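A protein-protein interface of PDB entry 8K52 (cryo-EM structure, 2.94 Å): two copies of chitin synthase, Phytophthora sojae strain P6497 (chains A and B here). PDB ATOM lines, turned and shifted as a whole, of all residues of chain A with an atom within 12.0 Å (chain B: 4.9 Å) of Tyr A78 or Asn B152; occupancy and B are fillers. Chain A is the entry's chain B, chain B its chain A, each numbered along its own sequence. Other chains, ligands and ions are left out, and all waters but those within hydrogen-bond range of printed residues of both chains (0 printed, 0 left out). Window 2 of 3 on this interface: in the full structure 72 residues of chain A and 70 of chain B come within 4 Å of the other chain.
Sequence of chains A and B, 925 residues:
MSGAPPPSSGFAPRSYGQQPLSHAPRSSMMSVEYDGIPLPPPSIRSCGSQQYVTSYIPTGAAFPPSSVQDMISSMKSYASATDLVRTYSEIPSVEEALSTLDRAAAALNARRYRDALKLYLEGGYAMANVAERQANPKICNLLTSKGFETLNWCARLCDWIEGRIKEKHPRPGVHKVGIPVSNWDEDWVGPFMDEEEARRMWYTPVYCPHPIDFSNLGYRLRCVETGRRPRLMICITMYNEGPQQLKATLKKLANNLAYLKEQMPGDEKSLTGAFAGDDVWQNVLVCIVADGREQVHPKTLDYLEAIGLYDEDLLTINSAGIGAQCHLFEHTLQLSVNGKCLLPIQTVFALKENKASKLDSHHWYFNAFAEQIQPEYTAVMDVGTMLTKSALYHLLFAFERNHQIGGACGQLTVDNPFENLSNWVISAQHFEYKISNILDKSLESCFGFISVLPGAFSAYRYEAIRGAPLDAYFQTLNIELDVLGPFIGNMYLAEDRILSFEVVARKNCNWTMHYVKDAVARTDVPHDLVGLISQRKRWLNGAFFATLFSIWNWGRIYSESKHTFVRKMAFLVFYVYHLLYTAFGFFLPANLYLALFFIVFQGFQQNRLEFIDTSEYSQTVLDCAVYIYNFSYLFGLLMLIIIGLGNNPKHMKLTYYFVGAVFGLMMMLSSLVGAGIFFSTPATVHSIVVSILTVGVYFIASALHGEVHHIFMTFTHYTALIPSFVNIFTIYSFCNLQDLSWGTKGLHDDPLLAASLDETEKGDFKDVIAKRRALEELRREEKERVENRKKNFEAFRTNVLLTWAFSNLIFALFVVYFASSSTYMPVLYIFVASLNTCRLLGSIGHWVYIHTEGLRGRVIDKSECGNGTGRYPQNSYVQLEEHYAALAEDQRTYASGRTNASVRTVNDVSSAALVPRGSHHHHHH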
ATOM      1  N   SER A  49      -1.616 -22.576  25.193  1.00  0.00           N
ATOM      2  CA  SER A  49      -2.104 -21.456  25.989  1.00  0.00           C
ATOM      3  C   SER A  49      -1.842 -20.130  25.285  1.00  0.00           C
ATOM      4  O   SER A  49      -0.714 -19.842  24.882  1.00  0.00           O
ATOM      5  CB  SER A  49      -1.451 -21.455  27.372  1.00  0.00           C
ATOM      6  OG  SER A  49      -1.980 -20.423  28.186  1.00  0.00           O
ATOM      7  N   GLN A  50      -2.890 -19.326  25.139  1.00  0.00           N
ATOM      8  CA  GLN A  50      -2.781 -18.022  24.506  1.00  0.00           C
ATOM      9  C   GLN A  50      -2.462 -16.968  25.566  1.00  0.00           C
ATOM     10  O   GLN A  50      -2.128 -17.286  26.711  1.00  0.00           O
ATOM     11  CB  GLN A  50      -4.061 -17.703  23.738  1.00  0.00           C
ATOM     12  CG  GLN A  50      -3.842 -16.918  22.452  1.00  0.00           C
ATOM     13  CD  GLN A  50      -2.609 -17.369  21.692  1.00  0.00           C
ATOM     14  OE1 GLN A  50      -2.465 -18.547  21.362  1.00  0.00           O
ATOM     15  NE2 GLN A  50      -1.712 -16.431  21.411  1.00  0.00           N
ATOM     16  N   GLN A  51      -2.556 -15.695  25.193  1.00  0.00           N
ATOM     17  CA  GLN A  51      -2.294 -14.596  26.115  1.00  0.00           C
ATOM     18  C   GLN A  51      -3.341 -14.533  27.222  1.00  0.00           C
ATOM     19  O   GLN A  51      -3.012 -14.321  28.390  1.00  0.00           O
ATOM     20  CB  GLN A  51      -2.249 -13.267  25.359  1.00  0.00           C
ATOM     21  CG  GLN A  51      -2.137 -12.043  26.248  1.00  0.00           C
ATOM     22  CD  GLN A  51      -2.327 -10.752  25.481  1.00  0.00           C
ATOM     23  OE1 GLN A  51      -3.236 -10.632  24.661  1.00  0.00           O
ATOM     24  NE2 GLN A  51      -1.465  -9.777  25.743  1.00  0.00           N
ATOM     25  N   SER A  77       1.429 -32.083  20.025  1.00  0.00           N
ATOM     26  CA  SER A  77       2.467 -31.215  20.568  1.00  0.00           C
ATOM     27  C   SER A  77       3.164 -31.874  21.753  1.00  0.00           C
ATOM     28  O   SER A  77       4.344 -31.633  22.003  1.00  0.00           O
ATOM     29  CB  SER A  77       1.875 -29.870  20.990  1.00  0.00           C
ATOM     30  OG  SER A  77       0.807 -30.047  21.905  1.00  0.00           O
ATOM     31  N   TYR A  78       2.418 -32.707  22.482  1.00  0.00           N
ATOM     32  CA  TYR A  78       2.986 -33.392  23.637  1.00  0.00           C
ATOM     33  C   TYR A  78       4.055 -34.395  23.224  1.00  0.00           C
ATOM     34  O   TYR A  78       5.047 -34.574  23.939  1.00  0.00           O
ATOM     35  CB  TYR A  78       1.881 -34.088  24.431  1.00  0.00           C
ATOM     36  CG  TYR A  78       0.818 -33.148  24.951  1.00  0.00           C
ATOM     37  CD1 TYR A  78       1.113 -31.821  25.238  1.00  0.00           C
ATOM     38  CD2 TYR A  78      -0.484 -33.587  25.154  1.00  0.00           C
ATOM     39  CE1 TYR A  78       0.143 -30.959  25.713  1.00  0.00           C
ATOM     40  CE2 TYR A  78      -1.461 -32.733  25.628  1.00  0.00           C
ATOM     41  CZ  TYR A  78      -1.142 -31.420  25.906  1.00  0.00           C
ATOM     42  OH  TYR A  78      -2.113 -30.567  26.378  1.00  0.00           O
ATOM     43  N   ALA A  79       3.868 -35.063  22.083  1.00  0.00           N
ATOM     44  CA  ALA A  79       4.871 -36.007  21.601  1.00  0.00           C
ATOM     45  C   ALA A  79       6.184 -35.299  21.291  1.00  0.00           C
ATOM     46  O   ALA A  79       7.267 -35.806  21.609  1.00  0.00           O
ATOM     47  CB  ALA A  79       4.347 -36.744  20.369  1.00  0.00           C
ATOM     48  N   SER A  80       6.107 -34.125  20.660  1.00  0.00           N
ATOM     49  CA  SER A  80       7.316 -33.360  20.371  1.00  0.00           C
ATOM     50  C   SER A  80       8.001 -32.905  21.654  1.00  0.00           C
ATOM     51  O   SER A  80       9.232 -32.955  21.760  1.00  0.00           O
ATOM     52  CB  SER A  80       6.979 -32.159  19.487  1.00  0.00           C
ATOM     53  OG  SER A  80       8.136 -31.392  19.207  1.00  0.00           O
ATOM     54  N   ALA A  81       7.220 -32.452  22.637  1.00  0.00           N
ATOM     55  CA  ALA A  81       7.798 -32.052  23.917  1.00  0.00           C
ATOM     56  C   ALA A  81       8.416 -33.242  24.638  1.00  0.00           C
ATOM     57  O   ALA A  81       9.495 -33.125  25.233  1.00  0.00           O
ATOM     58  CB  ALA A  81       6.734 -31.387  24.789  1.00  0.00           C
ATOM     59  N   THR A  82       7.745 -34.396  24.605  1.00  0.00           N
ATOM     60  CA  THR A  82       8.300 -35.596  25.221  1.00  0.00           C
ATOM     61  C   THR A  82       9.590 -36.025  24.531  1.00  0.00           C
ATOM     62  O   THR A  82      10.557 -36.414  25.196  1.00  0.00           O
ATOM     63  CB  THR A  82       7.273 -36.728  25.189  1.00  0.00           C
ATOM     64  OG1 THR A  82       6.052 -36.284  25.796  1.00  0.00           O
ATOM     65  CG2 THR A  82       7.793 -37.944  25.941  1.00  0.00           C
ATOM     66  N   ASP A  83       9.620 -35.962  23.197  1.00  0.00           N
ATOM     67  CA  ASP A  83      10.840 -36.295  22.467  1.00  0.00           C
ATOM     68  C   ASP A  83      11.964 -35.325  22.805  1.00  0.00           C
ATOM     69  O   ASP A  83      13.124 -35.731  22.946  1.00  0.00           O
ATOM     70  CB  ASP A  83      10.567 -36.301  20.963  1.00  0.00           C
ATOM     71  CG  ASP A  83       9.699 -37.467  20.533  1.00  0.00           C
ATOM     72  OD1 ASP A  83       9.311 -38.273  21.405  1.00  0.00           O
ATOM     73  OD2 ASP A  83       9.405 -37.578  19.324  1.00  0.00           O
ATOM     74  N   LEU A  84      11.641 -34.034  22.932  1.00  0.00           N
ATOM     75  CA  LEU A  84      12.647 -33.056  23.331  1.00  0.00           C
ATOM     76  C   LEU A  84      13.168 -33.344  24.733  1.00  0.00           C
ATOM     77  O   LEU A  84      14.367 -33.206  24.999  1.00  0.00           O
ATOM     78  CB  LEU A  84      12.065 -31.644  23.253  1.00  0.00           C
ATOM     79  CG  LEU A  84      13.031 -30.500  23.566  1.00  0.00           C
ATOM     80  CD1 LEU A  84      14.193 -30.499  22.586  1.00  0.00           C
ATOM     81  CD2 LEU A  84      12.308 -29.163  23.547  1.00  0.00           C
ATOM     82  N   VAL A  85      12.283 -33.743  25.640  1.00  0.00           N
ATOM     83  CA  VAL A  85      12.675 -34.084  27.001  1.00  0.00           C
ATOM     84  C   VAL A  85      13.486 -35.374  27.010  1.00  0.00           C
ATOM     85  O   VAL A  85      14.670 -35.371  27.350  1.00  0.00           O
ATOM     86  CB  VAL A  85      11.446 -34.207  27.917  1.00  0.00           C
ATOM     87  CG1 VAL A  85      11.803 -34.970  29.183  1.00  0.00           C
ATOM     88  CG2 VAL A  85      10.898 -32.830  28.255  1.00  0.00           C
ATOM     89  N   TYR B 125       1.671 -33.367  34.671  1.00  0.00           N
ATOM     90  CA  TYR B 125       1.238 -34.759  34.639  1.00  0.00           C
ATOM     91  C   TYR B 125       0.913 -35.279  36.031  1.00  0.00           C
ATOM     92  O   TYR B 125       0.005 -36.106  36.183  1.00  0.00           O
ATOM     93  CB  TYR B 125       2.301 -35.632  33.971  1.00  0.00           C
ATOM     94  CG  TYR B 125       2.434 -35.400  32.481  1.00  0.00           C
ATOM     95  CD1 TYR B 125       1.333 -35.512  31.644  1.00  0.00           C
ATOM     96  CD2 TYR B 125       3.658 -35.080  31.913  1.00  0.00           C
ATOM     97  CE1 TYR B 125       1.446 -35.306  30.283  1.00  0.00           C
ATOM     98  CE2 TYR B 125       3.782 -34.871  30.554  1.00  0.00           C
ATOM     99  CZ  TYR B 125       2.673 -34.986  29.744  1.00  0.00           C
ATOM    100  OH  TYR B 125       2.795 -34.779  28.390  1.00  0.00           O
ATOM    101  N   PHE B 148      -4.399 -29.175  32.926  1.00  0.00           N
ATOM    102  CA  PHE B 148      -4.603 -28.863  31.515  1.00  0.00           C
ATOM    103  C   PHE B 148      -3.948 -27.535  31.154  1.00  0.00           C
ATOM    104  O   PHE B 148      -3.271 -27.426  30.123  1.00  0.00           O
ATOM    105  CB  PHE B 148      -6.105 -28.848  31.213  1.00  0.00           C
ATOM    106  CG  PHE B 148      -6.447 -28.948  29.747  1.00  0.00           C
ATOM    107  CD1 PHE B 148      -6.106 -27.944  28.859  1.00  0.00           C
ATOM    108  CD2 PHE B 148      -7.121 -30.058  29.266  1.00  0.00           C
ATOM    109  CE1 PHE B 148      -6.426 -28.046  27.517  1.00  0.00           C
ATOM    110  CE2 PHE B 148      -7.445 -30.166  27.925  1.00  0.00           C
ATOM    111  CZ  PHE B 148      -7.096 -29.159  27.051  1.00  0.00           C
ATOM    112  N   GLU B 149      -4.115 -26.519  32.005  1.00  0.00           N
ATOM    113  CA  GLU B 149      -3.505 -25.222  31.735  1.00  0.00           C
ATOM    114  C   GLU B 149      -1.987 -25.305  31.803  1.00  0.00           C
ATOM    115  O   GLU B 149      -1.286 -24.661  31.014  1.00  0.00           O
ATOM    116  CB  GLU B 149      -4.045 -24.178  32.715  1.00  0.00           C
ATOM    117  CG  GLU B 149      -3.484 -22.774  32.531  1.00  0.00           C
ATOM    118  CD  GLU B 149      -2.235 -22.511  33.355  1.00  0.00           C
ATOM    119  OE1 GLU B 149      -1.766 -21.354  33.364  1.00  0.00           O
ATOM    120  OE2 GLU B 149      -1.734 -23.450  34.006  1.00  0.00           O
ATOM    121  N   THR B 150      -1.456 -26.092  32.742  1.00  0.00           N
ATOM    122  CA  THR B 150      -0.009 -26.241  32.845  1.00  0.00           C
ATOM    123  C   THR B 150       0.556 -26.963  31.630  1.00  0.00           C
ATOM    124  O   THR B 150       1.645 -26.631  31.160  1.00  0.00           O
ATOM    125  CB  THR B 150       0.352 -26.982  34.130  1.00  0.00           C
ATOM    126  OG1 THR B 150      -0.281 -26.342  35.243  1.00  0.00           O
ATOM    127  CG2 THR B 150       1.856 -26.965  34.345  1.00  0.00           C
ATOM    128  N   LEU B 151      -0.168 -27.955  31.105  1.00  0.00           N
ATOM    129  CA  LEU B 151       0.268 -28.609  29.875  1.00  0.00           C
ATOM    130  C   LEU B 151       0.231 -27.647  28.695  1.00  0.00           C
ATOM    131  O   LEU B 151       1.131 -27.662  27.845  1.00  0.00           O
ATOM    132  CB  LEU B 151      -0.591 -29.842  29.593  1.00  0.00           C
ATOM    133  CG  LEU B 151      -0.531 -31.019  30.572  1.00  0.00           C
ATOM    134  CD1 LEU B 151      -0.696 -32.333  29.825  1.00  0.00           C
ATOM    135  CD2 LEU B 151       0.773 -31.022  31.357  1.00  0.00           C
ATOM    136  N   ASN B 152      -0.806 -26.807  28.617  1.00  0.00           N
ATOM    137  CA  ASN B 152      -0.845 -25.802  27.556  1.00  0.00           C
ATOM    138  C   ASN B 152       0.338 -24.850  27.661  1.00  0.00           C
ATOM    139  O   ASN B 152       0.976 -24.518  26.653  1.00  0.00           O
ATOM    140  CB  ASN B 152      -2.156 -25.020  27.612  1.00  0.00           C
ATOM    141  CG  ASN B 152      -3.369 -25.893  27.382  1.00  0.00           C
ATOM    142  OD1 ASN B 152      -3.284 -26.940  26.743  1.00  0.00           O
ATOM    143  ND2 ASN B 152      -4.512 -25.454  27.892  1.00  0.00           N
ATOM    144  N   TRP B 153       0.652 -24.407  28.878  1.00  0.00           N
ATOM    145  CA  TRP B 153       1.790 -23.518  29.076  1.00  0.00           C
ATOM    146  C   TRP B 153       3.107 -24.217  28.765  1.00  0.00           C
ATOM    147  O   TRP B 153       4.028 -23.590  28.235  1.00  0.00           O
ATOM    148  CB  TRP B 153       1.786 -22.978  30.506  1.00  0.00           C
ATOM    149  CG  TRP B 153       3.145 -22.736  31.066  1.00  0.00           C
ATOM    150  CD1 TRP B 153       3.752 -23.429  32.068  1.00  0.00           C
ATOM    151  CD2 TRP B 153       4.070 -21.721  30.663  1.00  0.00           C
ATOM    152  NE1 TRP B 153       5.000 -22.913  32.313  1.00  0.00           N
ATOM    153  CE2 TRP B 153       5.218 -21.863  31.462  1.00  0.00           C
ATOM    154  CE3 TRP B 153       4.039 -20.710  29.700  1.00  0.00           C
ATOM    155  CZ2 TRP B 153       6.324 -21.031  31.330  1.00  0.00           C
ATOM    156  CZ3 TRP B 153       5.139 -19.886  29.571  1.00  0.00           C
ATOM    157  CH2 TRP B 153       6.265 -20.050  30.382  1.00  0.00           C
ATOM    158  N   CYS B 154       3.215 -25.508  29.087  1.00  0.00           N
ATOM    159  CA  CYS B 154       4.410 -26.268  28.739  1.00  0.00           C
ATOM    160  C   CYS B 154       4.585 -26.350  27.231  1.00  0.00           C
ATOM    161  O   CYS B 154       5.699 -26.200  26.718  1.00  0.00           O
ATOM    162  CB  CYS B 154       4.329 -27.672  29.333  1.00  0.00           C
ATOM    163  SG  CYS B 154       4.592 -27.756  31.107  1.00  0.00           S
ATOM    164  N   ALA B 155       3.495 -26.605  26.504  1.00  0.00           N
ATOM    165  CA  ALA B 155       3.575 -26.643  25.048  1.00  0.00           C
ATOM    166  C   ALA B 155       3.978 -25.286  24.490  1.00  0.00           C
ATOM    167  O   ALA B 155       4.802 -25.201  23.569  1.00  0.00           O
ATOM    168  CB  ALA B 155       2.240 -27.095  24.458  1.00  0.00           C
ATOM    169  N   ARG B 156       3.411 -24.211  25.042  1.00  0.00           N
ATOM    170  CA  ARG B 156       3.774 -22.873  24.586  1.00  0.00           C
ATOM    171  C   ARG B 156       5.245 -22.577  24.855  1.00  0.00           C
ATOM    172  O   ARG B 156       5.937 -22.011  24.005  1.00  0.00           O
ATOM    173  CB  ARG B 156       2.877 -21.830  25.253  1.00  0.00           C
ATOM    174  CG  ARG B 156       3.591 -20.553  25.659  1.00  0.00           C
ATOM    175  CD  ARG B 156       2.600 -19.439  25.940  1.00  0.00           C
ATOM    176  NE  ARG B 156       3.265 -18.219  26.377  1.00  0.00           N
ATOM    177  CZ  ARG B 156       3.390 -17.128  25.634  1.00  0.00           C
ATOM    178  NH1 ARG B 156       2.898 -17.068  24.407  1.00  0.00           N
ATOM    179  NH2 ARG B 156       4.023 -16.071  26.135  1.00  0.00           N
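No position is printed for both chains.
CB of Asn B152 touches N of Ser A49 (3.5 Å). CB of Ser A49 touches N of Trp B153, at 3.9 Å. Ser A49 touches Arg B156. Tyr A78 touches Leu B151. Tyr A78 touches Asn B152 (OH to OD1, 3.8 Å).
The backbone carbonyl oxygen (O) of Tyr A78 sits at hydrogen-bond distance from the side-chain hydroxyl (OG1) of Thr A82 (2.7 Å). O of Phe B148 lies close to ND2 of Asn B152, 3.2 Å away.
Of the 10 printed residues of chain B, 4 touch a printed residue of chain A. Hydrophobic or aromatic side chains of chain B within 4 Å of the printed part of chain A: Leu B151. Among the printed residues, no Asp or Glu carboxylate lies within 4 Å of a Lys or Arg side-chain nitrogen of the other chain.
Of the printed residues of chain B, Tyr A78 touches Leu B151 and Asn B152. Asn B152 touches just these residues of chain A: Ser A49 and Tyr A78. No residue of chain A comes within 4 Å of Phe B148. Trp B153 touches just one residue of chain A: Ser A49 (3.9 Å). Printed residues of chain B within 4 Å of Ser A49: Asn B152, Trp B153 and Arg B156. Of the printed residues of chain A, Arg B156 touches Ser A49. Leu A84 touches none of the printed residues of chain B. The nearest residue of chain B that does not touch Tyr A78 is Tyr B125 (4.1 Å). The nearest residue of chain A that does not touch Asn B152 is Gln A50 (6.3 Å).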
